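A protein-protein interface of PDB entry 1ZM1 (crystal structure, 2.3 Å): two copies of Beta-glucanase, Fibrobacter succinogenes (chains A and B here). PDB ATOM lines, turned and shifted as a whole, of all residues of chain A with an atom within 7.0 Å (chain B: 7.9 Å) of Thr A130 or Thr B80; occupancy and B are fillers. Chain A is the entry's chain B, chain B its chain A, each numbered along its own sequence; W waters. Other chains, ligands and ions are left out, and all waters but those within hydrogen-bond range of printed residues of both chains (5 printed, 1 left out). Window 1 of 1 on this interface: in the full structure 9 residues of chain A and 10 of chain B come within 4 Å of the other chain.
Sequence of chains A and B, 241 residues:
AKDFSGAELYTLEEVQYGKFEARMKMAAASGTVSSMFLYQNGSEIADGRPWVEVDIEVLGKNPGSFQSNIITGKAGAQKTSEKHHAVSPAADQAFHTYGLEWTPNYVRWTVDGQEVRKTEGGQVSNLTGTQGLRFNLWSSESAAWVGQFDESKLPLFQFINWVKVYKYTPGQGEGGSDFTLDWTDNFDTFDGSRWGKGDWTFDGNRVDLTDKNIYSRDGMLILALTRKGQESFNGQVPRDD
The side-chain amino group (NZ) of Lys B83 lies within hydrogen-bond range of the side-chain amide oxygen (OE1) of Gln A16 (2.7 Å).
O of Gln B78 sits at hydrogen-bond distance from N of Glu A14, 3.0 Å away.
The backbone NH of Thr B80 lies within hydrogen-bond range of the backbone carbonyl oxygen of Glu A14, 2.9 Å away.
O of Thr B80 is in hydrogen-bond range of N of Gln A16 (3.1 Å).
The side-chain hydroxyl of Thr B72 sits at hydrogen-bond distance from the side-chain amide nitrogen of Gln B123 (3.2 Å).
The backbone NH of Thr B72 sits at hydrogen-bond distance from the backbone carbonyl oxygen of Lys B79.
The side-chain hydroxyl (OG) of Ser B81 lies within hydrogen-bond range of the guanidinium group (NH1) of Arg B117 (2.9 Å).
The backbone NH (N) of Ser B68 lies within hydrogen-bond range of the backbone carbonyl oxygen (O) of Lys B83, at 2.9 Å.
OG of Ser B81 is in hydrogen-bond range of OE1 of Gln B123 (2.8 Å).
The side-chain carboxylate (OE1) of Glu A14 sits at hydrogen-bond distance from the backbone NH (N) of Asn A41 (2.9 Å).
Among the printed residues, merely in contact across the chains: Glu A13 with Gln B78 (3.1 Å), Glu A14 with Lys B79 (3.2 Å), Val A15 with Thr B80 (3.1 Å), Gln A16 with Ser B81 (3.6 Å), Tyr A17 with Lys B83 (3.5 Å), Gly A129 with Gly B122 (3.7 Å), Thr A130 with Lys B79 (3.5 Å), Thr A130 with Thr B80 (3.4 Å) and Thr A130 with Gln B123 (3.8 Å).
Printed residues of chain B within 4 Å of Glu A14: Gln B78 (3.0 Å), Lys B79 (3.2 Å) and Thr B80 (2.9 Å).
Of the printed residues of chain B, Gln A16 touches Thr B80, Ser B81 and Lys B83.
Asn A41 touches none of the printed residues of chain B.
Ser A43 touches none of the printed residues of chain B.
Of chain B, only Gly B122 comes within 4 Å of Gly A129.
Of chain B, only Lys B79 (3.5 Å), Thr B80 (3.4 Å) and Gln B123 (3.8 Å) come within 4 Å of Thr A130.
Of chain A, only Glu A14, Val A15, Gln A16 and Thr A130 come within 4 Å of Thr B80.
Of the printed residues of chain A, Lys B83 touches Gln A16 (2.7 Å) and Tyr A17 (3.5 Å).
The nearest residue of chain B that does not touch Thr A130 is Ser B81 (5.2 Å).
Of the 17 printed residues of chain A, 7 touch a printed residue of chain B.
Among the printed residues, no Asp or Glu carboxylate lies within 4 Å of a Lys or Arg side-chain nitrogen of the other chain.
No position is printed for both chains.
Water W3 lies within hydrogen-bond range of O of Asn A41, NZ of Lys B79 and OE2 of Glu A14.
Water W4 lies within hydrogen-bond range of the side-chain carboxylate of Glu A13 (2.7 Å), the backbone NH of Gln B78 (2.9 Å) and the backbone NH of Ala B77 (3.5 Å).
Water W5 lies within hydrogen-bond range of the side-chain carboxylate (OE2) of Glu A13 and the side-chain amide nitrogen (NE2) of Gln B78.
Water W2 lies within hydrogen-bond range of the side-chain amide oxygen of Asn A41 and the side-chain amino group of Lys B79.
Water W1 bridges N of Gly A129 (3.1 Å) and O of Gly B121 (3.5 Å).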
ATOM      1  N   GLU A  13     -22.233  13.900 -18.717  1.00  0.00           N
ATOM      2  CA  GLU A  13     -22.514  14.251 -20.103  1.00  0.00           C
ATOM      3  C   GLU A  13     -21.665  13.459 -21.088  1.00  0.00           C
ATOM      4  O   GLU A  13     -20.672  12.839 -20.715  1.00  0.00           O
ATOM      5  CB  GLU A  13     -22.283  15.757 -20.329  1.00  0.00           C
ATOM      6  CG  GLU A  13     -23.094  16.665 -19.410  1.00  0.00           C
ATOM      7  CD  GLU A  13     -22.993  18.145 -19.781  1.00  0.00           C
ATOM      8  OE1 GLU A  13     -21.860  18.658 -19.910  1.00  0.00           O
ATOM      9  OE2 GLU A  13     -24.051  18.801 -19.932  1.00  0.00           O
ATOM     10  N   GLU A  14     -22.084  13.469 -22.348  1.00  0.00           N
ATOM     11  CA  GLU A  14     -21.349  12.804 -23.419  1.00  0.00           C
ATOM     12  C   GLU A  14     -21.225  13.816 -24.557  1.00  0.00           C
ATOM     13  O   GLU A  14     -22.045  14.724 -24.674  1.00  0.00           O
ATOM     14  CB  GLU A  14     -22.089  11.553 -23.915  1.00  0.00           C
ATOM     15  CG  GLU A  14     -22.157  10.405 -22.916  1.00  0.00           C
ATOM     16  CD  GLU A  14     -22.620   9.107 -23.554  1.00  0.00           C
ATOM     17  OE1 GLU A  14     -22.673   8.076 -22.853  1.00  0.00           O
ATOM     18  OE2 GLU A  14     -22.930   9.117 -24.763  1.00  0.00           O
ATOM     19  N   VAL A  15     -20.196  13.667 -25.381  1.00  0.00           N
ATOM     20  CA  VAL A  15     -19.991  14.575 -26.505  1.00  0.00           C
ATOM     21  C   VAL A  15     -19.461  13.849 -27.731  1.00  0.00           C
ATOM     22  O   VAL A  15     -19.049  12.690 -27.659  1.00  0.00           O
ATOM     23  CB  VAL A  15     -18.976  15.686 -26.173  1.00  0.00           C
ATOM     24  CG1 VAL A  15     -19.503  16.553 -25.063  1.00  0.00           C
ATOM     25  CG2 VAL A  15     -17.635  15.064 -25.784  1.00  0.00           C
ATOM     26  N   GLN A  16     -19.482  14.538 -28.864  1.00  0.00           N
ATOM     27  CA  GLN A  16     -18.953  13.956 -30.080  1.00  0.00           C
ATOM     28  C   GLN A  16     -17.626  14.627 -30.376  1.00  0.00           C
ATOM     29  O   GLN A  16     -17.583  15.823 -30.679  1.00  0.00           O
ATOM     30  CB  GLN A  16     -19.901  14.156 -31.259  1.00  0.00           C
ATOM     31  CG  GLN A  16     -19.403  13.458 -32.526  1.00  0.00           C
ATOM     32  CD  GLN A  16     -20.277  13.723 -33.734  1.00  0.00           C
ATOM     33  OE1 GLN A  16     -20.632  14.867 -34.010  1.00  0.00           O
ATOM     34  NE2 GLN A  16     -20.617  12.668 -34.468  1.00  0.00           N
ATOM     35  N   TYR A  17     -16.549  13.853 -30.254  1.00  0.00           N
ATOM     36  CA  TYR A  17     -15.204  14.329 -30.537  1.00  0.00           C
ATOM     37  C   TYR A  17     -14.627  15.212 -29.435  1.00  0.00           C
ATOM     38  O   TYR A  17     -15.353  15.693 -28.563  1.00  0.00           O
ATOM     39  CB  TYR A  17     -15.199  15.099 -31.863  1.00  0.00           C
ATOM     40  CG  TYR A  17     -15.844  14.358 -33.020  1.00  0.00           C
ATOM     41  CD1 TYR A  17     -16.555  15.044 -33.999  1.00  0.00           C
ATOM     42  CD2 TYR A  17     -15.725  12.977 -33.147  1.00  0.00           C
ATOM     43  CE1 TYR A  17     -17.135  14.372 -35.080  1.00  0.00           C
ATOM     44  CE2 TYR A  17     -16.298  12.298 -34.216  1.00  0.00           C
ATOM     45  CZ  TYR A  17     -17.003  13.003 -35.177  1.00  0.00           C
ATOM     46  OH  TYR A  17     -17.589  12.328 -36.218  1.00  0.00           O
ATOM     47  N   TYR A  39     -16.484   6.255 -23.515  1.00  0.00           N
ATOM     48  CA  TYR A  39     -17.535   5.254 -23.596  1.00  0.00           C
ATOM     49  C   TYR A  39     -18.913   5.796 -23.971  1.00  0.00           C
ATOM     50  O   TYR A  39     -19.359   6.826 -23.448  1.00  0.00           O
ATOM     51  CB  TYR A  39     -17.630   4.516 -22.253  1.00  0.00           C
ATOM     52  CG  TYR A  39     -18.544   3.310 -22.248  1.00  0.00           C
ATOM     53  CD1 TYR A  39     -18.190   2.141 -22.913  1.00  0.00           C
ATOM     54  CD2 TYR A  39     -19.749   3.331 -21.551  1.00  0.00           C
ATOM     55  CE1 TYR A  39     -19.011   1.015 -22.879  1.00  0.00           C
ATOM     56  CE2 TYR A  39     -20.579   2.213 -21.511  1.00  0.00           C
ATOM     57  CZ  TYR A  39     -20.205   1.058 -22.178  1.00  0.00           C
ATOM     58  OH  TYR A  39     -21.027  -0.051 -22.154  1.00  0.00           O
ATOM     59  N   GLN A  40     -19.576   5.090 -24.885  1.00  0.00           N
ATOM     60  CA  GLN A  40     -20.919   5.456 -25.325  1.00  0.00           C
ATOM     61  C   GLN A  40     -21.853   4.611 -24.478  1.00  0.00           C
ATOM     62  O   GLN A  40     -22.108   3.441 -24.781  1.00  0.00           O
ATOM     63  CB  GLN A  40     -21.102   5.145 -26.812  1.00  0.00           C
ATOM     64  CG  GLN A  40     -22.534   5.321 -27.321  1.00  0.00           C
ATOM     65  CD  GLN A  40     -22.607   5.491 -28.835  1.00  0.00           C
ATOM     66  OE1 GLN A  40     -22.149   6.496 -29.373  1.00  0.00           O
ATOM     67  NE2 GLN A  40     -23.176   4.508 -29.524  1.00  0.00           N
ATOM     68  N   ASN A  41     -22.342   5.202 -23.398  1.00  0.00           N
ATOM     69  CA  ASN A  41     -23.222   4.479 -22.504  1.00  0.00           C
ATOM     70  C   ASN A  41     -24.355   3.830 -23.276  1.00  0.00           C
ATOM     71  O   ASN A  41     -24.931   4.438 -24.183  1.00  0.00           O
ATOM     72  CB  ASN A  41     -23.805   5.404 -21.446  1.00  0.00           C
ATOM     73  CG  ASN A  41     -24.378   4.639 -20.275  1.00  0.00           C
ATOM     74  OD1 ASN A  41     -25.257   5.125 -19.568  1.00  0.00           O
ATOM     75  ND2 ASN A  41     -23.865   3.435 -20.055  1.00  0.00           N
ATOM     76  N   SER A  43     -23.832   0.991 -24.786  1.00  0.00           N
ATOM     77  CA  SER A  43     -23.139   0.084 -25.686  1.00  0.00           C
ATOM     78  C   SER A  43     -23.254  -1.360 -25.200  1.00  0.00           C
ATOM     79  O   SER A  43     -23.191  -2.298 -26.001  1.00  0.00           O
ATOM     80  CB  SER A  43     -21.650   0.460 -25.804  1.00  0.00           C
ATOM     81  OG  SER A  43     -21.448   1.634 -26.573  1.00  0.00           O
ATOM     82  N   VAL A  52     -19.542   1.557 -28.965  1.00  0.00           N
ATOM     83  CA  VAL A  52     -18.610   2.655 -29.236  1.00  0.00           C
ATOM     84  C   VAL A  52     -17.737   2.887 -27.993  1.00  0.00           C
ATOM     85  O   VAL A  52     -18.237   3.218 -26.914  1.00  0.00           O
ATOM     86  CB  VAL A  52     -19.371   3.949 -29.610  1.00  0.00           C
ATOM     87  CG1 VAL A  52     -18.395   5.096 -29.812  1.00  0.00           C
ATOM     88  CG2 VAL A  52     -20.166   3.724 -30.896  1.00  0.00           C
ATOM     89  N   TRP A 102     -10.049  12.316 -30.181  1.00  0.00           N
ATOM     90  CA  TRP A 102     -11.045  11.656 -31.002  1.00  0.00           C
ATOM     91  C   TRP A 102     -11.696  12.628 -31.971  1.00  0.00           C
ATOM     92  O   TRP A 102     -12.386  13.563 -31.570  1.00  0.00           O
ATOM     93  CB  TRP A 102     -12.096  10.995 -30.100  1.00  0.00           C
ATOM     94  CG  TRP A 102     -13.324  10.499 -30.807  1.00  0.00           C
ATOM     95  CD1 TRP A 102     -13.384   9.877 -32.020  1.00  0.00           C
ATOM     96  CD2 TRP A 102     -14.667  10.568 -30.325  1.00  0.00           C
ATOM     97  NE1 TRP A 102     -14.683   9.556 -32.326  1.00  0.00           N
ATOM     98  CE2 TRP A 102     -15.492   9.971 -31.301  1.00  0.00           C
ATOM     99  CE3 TRP A 102     -15.256  11.078 -29.159  1.00  0.00           C
ATOM    100  CZ2 TRP A 102     -16.880   9.869 -31.147  1.00  0.00           C
ATOM    101  CZ3 TRP A 102     -16.643  10.975 -29.007  1.00  0.00           C
ATOM    102  CH2 TRP A 102     -17.434  10.377 -29.997  1.00  0.00           C
ATOM    103  N   LEU A 127     -17.090   4.951 -34.973  1.00  0.00           N
ATOM    104  CA  LEU A 127     -17.275   5.510 -33.642  1.00  0.00           C
ATOM    105  C   LEU A 127     -18.284   6.623 -33.846  1.00  0.00           C
ATOM    106  O   LEU A 127     -17.925   7.802 -33.915  1.00  0.00           O
ATOM    107  CB  LEU A 127     -15.967   6.090 -33.103  1.00  0.00           C
ATOM    108  CG  LEU A 127     -14.869   5.091 -32.742  1.00  0.00           C
ATOM    109  CD1 LEU A 127     -13.644   5.842 -32.260  1.00  0.00           C
ATOM    110  CD2 LEU A 127     -15.373   4.140 -31.666  1.00  0.00           C
ATOM    111  N   THR A 128     -19.545   6.229 -33.986  1.00  0.00           N
ATOM    112  CA  THR A 128     -20.641   7.163 -34.196  1.00  0.00           C
ATOM    113  C   THR A 128     -21.209   7.582 -32.845  1.00  0.00           C
ATOM    114  O   THR A 128     -20.929   6.952 -31.822  1.00  0.00           O
ATOM    115  CB  THR A 128     -21.767   6.508 -34.997  1.00  0.00           C
ATOM    116  OG1 THR A 128     -22.108   5.260 -34.391  1.00  0.00           O
ATOM    117  CG2 THR A 128     -21.344   6.264 -36.431  1.00  0.00           C
ATOM    118  N   GLY A 129     -22.010   8.643 -32.852  1.00  0.00           N
ATOM    119  CA  GLY A 129     -22.611   9.122 -31.623  1.00  0.00           C
ATOM    120  C   GLY A 129     -21.658   9.841 -30.684  1.00  0.00           C
ATOM    121  O   GLY A 129     -20.626  10.379 -31.104  1.00  0.00           O
ATOM    122  N   THR A 130     -22.016   9.840 -29.402  1.00  0.00           N
ATOM    123  CA  THR A 130     -21.234  10.500 -28.362  1.00  0.00           C
ATOM    124  C   THR A 130     -20.597   9.488 -27.426  1.00  0.00           C
ATOM    125  O   THR A 130     -20.879   8.290 -27.498  1.00  0.00           O
ATOM    126  CB  THR A 130     -22.132  11.424 -27.506  1.00  0.00           C
ATOM    127  OG1 THR A 130     -23.193  10.649 -26.927  1.00  0.00           O
ATOM    128  CG2 THR A 130     -22.742  12.524 -28.356  1.00  0.00           C
ATOM    129  N   GLN A 131     -19.728   9.977 -26.548  1.00  0.00           N
ATOM    130  CA  GLN A 131     -19.072   9.131 -25.552  1.00  0.00           C
ATOM    131  C   GLN A 131     -18.770  10.011 -24.342  1.00  0.00           C
ATOM    132  O   GLN A 131     -18.601  11.225 -24.470  1.00  0.00           O
ATOM    133  CB  GLN A 131     -17.746   8.541 -26.065  1.00  0.00           C
ATOM    134  CG  GLN A 131     -17.803   7.751 -27.368  1.00  0.00           C
ATOM    135  CD  GLN A 131     -16.455   7.115 -27.717  1.00  0.00           C
ATOM    136  OE1 GLN A 131     -16.043   6.144 -27.096  1.00  0.00           O
ATOM    137  NE2 GLN A 131     -15.756   7.681 -28.694  1.00  0.00           N
ATOM    138  N   GLY A 132     -18.734   9.404 -23.164  1.00  0.00           N
ATOM    139  CA  GLY A 132     -18.399  10.153 -21.972  1.00  0.00           C
ATOM    140  C   GLY A 132     -16.970   9.760 -21.623  1.00  0.00           C
ATOM    141  O   GLY A 132     -16.430   8.808 -22.193  1.00  0.00           O
ATOM    142  N   ASP B  55     -30.145  21.999 -33.004  1.00  0.00           N
ATOM    143  CA  ASP B  55     -29.942  23.431 -33.055  1.00  0.00           C
ATOM    144  C   ASP B  55     -29.081  24.059 -34.118  1.00  0.00           C
ATOM    145  O   ASP B  55     -28.213  23.431 -34.730  1.00  0.00           O
ATOM    146  CB  ASP B  55     -29.374  23.917 -31.720  1.00  0.00           C
ATOM    147  CG  ASP B  55     -30.160  23.431 -30.538  1.00  0.00           C
ATOM    148  OD1 ASP B  55     -31.328  23.840 -30.380  1.00  0.00           O
ATOM    149  OD2 ASP B  55     -29.596  22.636 -29.766  1.00  0.00           O
ATOM    150  N   GLN B  67     -23.549  27.871 -34.519  1.00  0.00           N
ATOM    151  CA  GLN B  67     -23.275  26.593 -33.893  1.00  0.00           C
ATOM    152  C   GLN B  67     -24.383  25.584 -34.198  1.00  0.00           C
ATOM    153  O   GLN B  67     -25.573  25.892 -34.097  1.00  0.00           O
ATOM    154  CB  GLN B  67     -23.128  26.786 -32.382  1.00  0.00           C
ATOM    155  CG  GLN B  67     -22.961  25.501 -31.621  1.00  0.00           C
ATOM    156  CD  GLN B  67     -22.680  25.728 -30.148  1.00  0.00           C
ATOM    157  OE1 GLN B  67     -21.614  26.205 -29.776  1.00  0.00           O
ATOM    158  NE2 GLN B  67     -23.641  25.385 -29.305  1.00  0.00           N
ATOM    159  N   SER B  68     -23.978  24.384 -34.594  1.00  0.00           N
ATOM    160  CA  SER B  68     -24.925  23.314 -34.892  1.00  0.00           C
ATOM    161  C   SER B  68     -24.908  22.416 -33.671  1.00  0.00           C
ATOM    162  O   SER B  68     -23.914  22.376 -32.942  1.00  0.00           O
ATOM    163  CB  SER B  68     -24.483  22.515 -36.119  1.00  0.00           C
ATOM    164  OG  SER B  68     -23.190  21.968 -35.917  1.00  0.00           O
ATOM    165  N   ASN B  69     -25.994  21.690 -33.440  1.00  0.00           N
ATOM    166  CA  ASN B  69     -26.037  20.821 -32.275  1.00  0.00           C
ATOM    167  C   ASN B  69     -27.244  19.899 -32.272  1.00  0.00           C
ATOM    168  O   ASN B  69     -28.310  20.228 -32.804  1.00  0.00           O
ATOM    169  CB  ASN B  69     -26.071  21.684 -31.008  1.00  0.00           C
ATOM    170  CG  ASN B  69     -25.460  20.994 -29.803  1.00  0.00           C
ATOM    171  OD1 ASN B  69     -25.132  19.808 -29.841  1.00  0.00           O
ATOM    172  ND2 ASN B  69     -25.309  21.743 -28.716  1.00  0.00           N
ATOM    173  N   ILE B  70     -27.049  18.737 -31.668  1.00  0.00           N
ATOM    174  CA  ILE B  70     -28.103  17.753 -31.494  1.00  0.00           C
ATOM    175  C   ILE B  70     -28.002  17.434 -30.006  1.00  0.00           C
ATOM    176  O   ILE B  70     -26.906  17.176 -29.506  1.00  0.00           O
ATOM    177  CB  ILE B  70     -27.836  16.454 -32.271  1.00  0.00           C
ATOM    178  CG1 ILE B  70     -27.775  16.734 -33.771  1.00  0.00           C
ATOM    179  CG2 ILE B  70     -28.920  15.447 -31.965  1.00  0.00           C
ATOM    180  CD1 ILE B  70     -27.381  15.512 -34.583  1.00  0.00           C
ATOM    181  N   ILE B  71     -29.127  17.461 -29.301  1.00  0.00           N
ATOM    182  CA  ILE B  71     -29.108  17.156 -27.878  1.00  0.00           C
ATOM    183  C   ILE B  71     -29.968  15.947 -27.540  1.00  0.00           C
ATOM    184  O   ILE B  71     -31.198  16.009 -27.596  1.00  0.00           O
ATOM    185  CB  ILE B  71     -29.602  18.344 -27.026  1.00  0.00           C
ATOM    186  CG1 ILE B  71     -28.835  19.616 -27.402  1.00  0.00           C
ATOM    187  CG2 ILE B  71     -29.393  18.034 -25.546  1.00  0.00           C
ATOM    188  CD1 ILE B  71     -29.198  20.818 -26.581  1.00  0.00           C
ATOM    189  N   THR B  72     -29.306  14.844 -27.204  1.00  0.00           N
ATOM    190  CA  THR B  72     -29.994  13.625 -26.818  1.00  0.00           C
ATOM    191  C   THR B  72     -29.644  13.355 -25.355  1.00  0.00           C
ATOM    192  O   THR B  72     -29.175  14.251 -24.651  1.00  0.00           O
ATOM    193  CB  THR B  72     -29.581  12.428 -27.707  1.00  0.00           C
ATOM    194  OG1 THR B  72     -28.174  12.192 -27.585  1.00  0.00           O
ATOM    195  CG2 THR B  72     -29.932  12.714 -29.168  1.00  0.00           C
ATOM    196  N   GLY B  73     -29.863  12.130 -24.893  1.00  0.00           N
ATOM    197  CA  GLY B  73     -29.586  11.826 -23.503  1.00  0.00           C
ATOM    198  C   GLY B  73     -30.760  12.315 -22.675  1.00  0.00           C
ATOM    199  O   GLY B  73     -31.909  12.014 -23.000  1.00  0.00           O
ATOM    200  N   ALA B  77     -28.093  14.943 -17.868  1.00  0.00           N
ATOM    201  CA  ALA B  77     -27.193  13.970 -18.483  1.00  0.00           C
ATOM    202  C   ALA B  77     -27.298  14.089 -19.993  1.00  0.00           C
ATOM    203  O   ALA B  77     -27.676  13.147 -20.683  1.00  0.00           O
ATOM    204  CB  ALA B  77     -27.567  12.560 -18.041  1.00  0.00           C
ATOM    205  N   GLN B  78     -26.968  15.267 -20.496  1.00  0.00           N
ATOM    206  CA  GLN B  78     -27.037  15.523 -21.920  1.00  0.00           C
ATOM    207  C   GLN B  78     -25.867  14.950 -22.706  1.00  0.00           C
ATOM    208  O   GLN B  78     -24.777  14.738 -22.176  1.00  0.00           O
ATOM    209  CB  GLN B  78     -27.141  17.027 -22.171  1.00  0.00           C
ATOM    210  CG  GLN B  78     -28.484  17.601 -21.808  1.00  0.00           C
ATOM    211  CD  GLN B  78     -28.572  19.086 -22.078  1.00  0.00           C
ATOM    212  OE1 GLN B  78     -29.659  19.668 -22.077  1.00  0.00           O
ATOM    213  NE2 GLN B  78     -27.425  19.713 -22.312  1.00  0.00           N
ATOM    214  N   LYS B  79     -26.135  14.680 -23.974  1.00  0.00           N
ATOM    215  CA  LYS B  79     -25.149  14.167 -24.911  1.00  0.00           C
ATOM    216  C   LYS B  79     -25.234  15.187 -26.037  1.00  0.00           C
ATOM    217  O   LYS B  79     -26.295  15.384 -26.631  1.00  0.00           O
ATOM    218  CB  LYS B  79     -25.550  12.765 -25.378  1.00  0.00           C
ATOM    219  CG  LYS B  79     -25.645  11.771 -24.219  1.00  0.00           C
ATOM    220  CD  LYS B  79     -26.211  10.431 -24.654  1.00  0.00           C
ATOM    221  CE  LYS B  79     -26.442   9.521 -23.462  1.00  0.00           C
ATOM    222  NZ  LYS B  79     -26.927   8.173 -23.879  1.00  0.00           N
ATOM    223  N   THR B  80     -24.120  15.853 -26.311  1.00  0.00           N
ATOM    224  CA  THR B  80     -24.096  16.903 -27.317  1.00  0.00           C
ATOM    225  C   THR B  80     -23.058  16.712 -28.420  1.00  0.00           C
ATOM    226  O   THR B  80     -22.204  15.833 -28.341  1.00  0.00           O
ATOM    227  CB  THR B  80     -23.831  18.247 -26.642  1.00  0.00           C
ATOM    228  OG1 THR B  80     -22.609  18.152 -25.905  1.00  0.00           O
ATOM    229  CG2 THR B  80     -24.967  18.605 -25.679  1.00  0.00           C
ATOM    230  N   SER B  81     -23.134  17.570 -29.434  1.00  0.00           N
ATOM    231  CA  SER B  81     -22.237  17.523 -30.581  1.00  0.00           C
ATOM    232  C   SER B  81     -22.149  18.914 -31.211  1.00  0.00           C
ATOM    233  O   SER B  81     -22.533  19.115 -32.363  1.00  0.00           O
ATOM    234  CB  SER B  81     -22.766  16.522 -31.614  1.00  0.00           C
ATOM    235  OG  SER B  81     -24.082  16.867 -32.026  1.00  0.00           O
ATOM    236  N   GLU B  82     -21.642  19.867 -30.442  1.00  0.00           N
ATOM    237  CA  GLU B  82     -21.507  21.240 -30.906  1.00  0.00           C
ATOM    238  C   GLU B  82     -20.437  21.391 -31.978  1.00  0.00           C
ATOM    239  O   GLU B  82     -19.321  20.904 -31.820  1.00  0.00           O
ATOM    240  CB  GLU B  82     -21.147  22.162 -29.740  1.00  0.00           C
ATOM    241  CG  GLU B  82     -22.142  22.180 -28.603  1.00  0.00           C
ATOM    242  CD  GLU B  82     -21.651  23.014 -27.436  1.00  0.00           C
ATOM    243  OE1 GLU B  82     -20.518  22.766 -26.970  1.00  0.00           O
ATOM    244  OE2 GLU B  82     -22.391  23.917 -26.980  1.00  0.00           O
ATOM    245  N   LYS B  83     -20.787  22.070 -33.065  1.00  0.00           N
ATOM    246  CA  LYS B  83     -19.847  22.335 -34.152  1.00  0.00           C
ATOM    247  C   LYS B  83     -20.059  23.775 -34.596  1.00  0.00           C
ATOM    248  O   LYS B  83     -21.097  24.379 -34.301  1.00  0.00           O
ATOM    249  CB  LYS B  83     -20.078  21.380 -35.322  1.00  0.00           C
ATOM    250  CG  LYS B  83     -19.991  19.920 -34.925  1.00  0.00           C
ATOM    251  CD  LYS B  83     -20.184  18.983 -36.119  1.00  0.00           C
ATOM    252  CE  LYS B  83     -20.421  17.564 -35.646  1.00  0.00           C
ATOM    253  NZ  LYS B  83     -19.323  17.099 -34.761  1.00  0.00           N
ATOM    254  N   ARG B 117     -23.514  20.564 -42.740  1.00  0.00           N
ATOM    255  CA  ARG B 117     -23.362  19.465 -41.788  1.00  0.00           C
ATOM    256  C   ARG B 117     -24.419  18.373 -41.945  1.00  0.00           C
ATOM    257  O   ARG B 117     -25.595  18.662 -42.122  1.00  0.00           O
ATOM    258  CB  ARG B 117     -23.424  19.979 -40.343  1.00  0.00           C
ATOM    259  CG  ARG B 117     -23.466  18.852 -39.301  1.00  0.00           C
ATOM    260  CD  ARG B 117     -23.678  19.329 -37.857  1.00  0.00           C
ATOM    261  NE  ARG B 117     -23.790  18.179 -36.956  1.00  0.00           N
ATOM    262  CZ  ARG B 117     -23.892  18.251 -35.631  1.00  0.00           C
ATOM    263  NH1 ARG B 117     -23.991  17.138 -34.912  1.00  0.00           N
ATOM    264  NH2 ARG B 117     -23.889  19.433 -35.022  1.00  0.00           N
ATOM    265  N   GLY B 121     -26.880   8.315 -38.195  1.00  0.00           N
ATOM    266  CA  GLY B 121     -26.822   7.379 -37.091  1.00  0.00           C
ATOM    267  C   GLY B 121     -26.460   8.085 -35.800  1.00  0.00           C
ATOM    268  O   GLY B 121     -26.650   9.298 -35.675  1.00  0.00           O
ATOM    269  N   GLY B 122     -25.942   7.329 -34.835  1.00  0.00           N
ATOM    270  CA  GLY B 122     -25.566   7.919 -33.562  1.00  0.00           C
ATOM    271  C   GLY B 122     -26.734   8.605 -32.884  1.00  0.00           C
ATOM    272  O   GLY B 122     -27.787   7.992 -32.680  1.00  0.00           O
ATOM    273  N   GLN B 123     -26.551   9.875 -32.534  1.00  0.00           N
ATOM    274  CA  GLN B 123     -27.592  10.653 -31.864  1.00  0.00           C
ATOM    275  C   GLN B 123     -28.903  10.712 -32.647  1.00  0.00           C
ATOM    276  O   GLN B 123     -29.980  10.782 -32.066  1.00  0.00           O
ATOM    277  CB  GLN B 123     -27.121  12.090 -31.629  1.00  0.00           C
ATOM    278  CG  GLN B 123     -25.992  12.269 -30.648  1.00  0.00           C
ATOM    279  CD  GLN B 123     -25.763  13.737 -30.340  1.00  0.00           C
ATOM    280  OE1 GLN B 123     -25.152  14.472 -31.131  1.00  0.00           O
ATOM    281  NE2 GLN B 123     -26.283  14.184 -29.202  1.00  0.00           N
ATOM    282  N   ASN B 126     -31.674   8.527 -31.726  1.00  0.00           N
ATOM    283  CA  ASN B 126     -32.363   8.775 -30.467  1.00  0.00           C
ATOM    284  C   ASN B 126     -33.225  10.023 -30.514  1.00  0.00           C
ATOM    285  O   ASN B 126     -33.649  10.534 -29.476  1.00  0.00           O
ATOM    286  CB  ASN B 126     -31.356   8.863 -29.322  1.00  0.00           C
ATOM    287  CG  ASN B 126     -30.519   7.610 -29.204  1.00  0.00           C
ATOM    288  OD1 ASN B 126     -31.038   6.517 -28.961  1.00  0.00           O
ATOM    289  ND2 ASN B 126     -29.216   7.756 -29.394  1.00  0.00           N
HETATM  290  O   HOH W   1     -23.192   9.630 -35.572  1.00  0.00           O
HETATM  291  O   HOH W   2     -27.293   6.935 -20.989  1.00  0.00           O
HETATM  292  O   HOH W   3     -24.866   6.947 -25.142  1.00  0.00           O
HETATM  293  O   HOH W   4     -26.331  17.711 -19.009  1.00  0.00           O
HETATM  294  O   HOH W   5     -24.696  20.468 -22.055  1.00  0.00           O
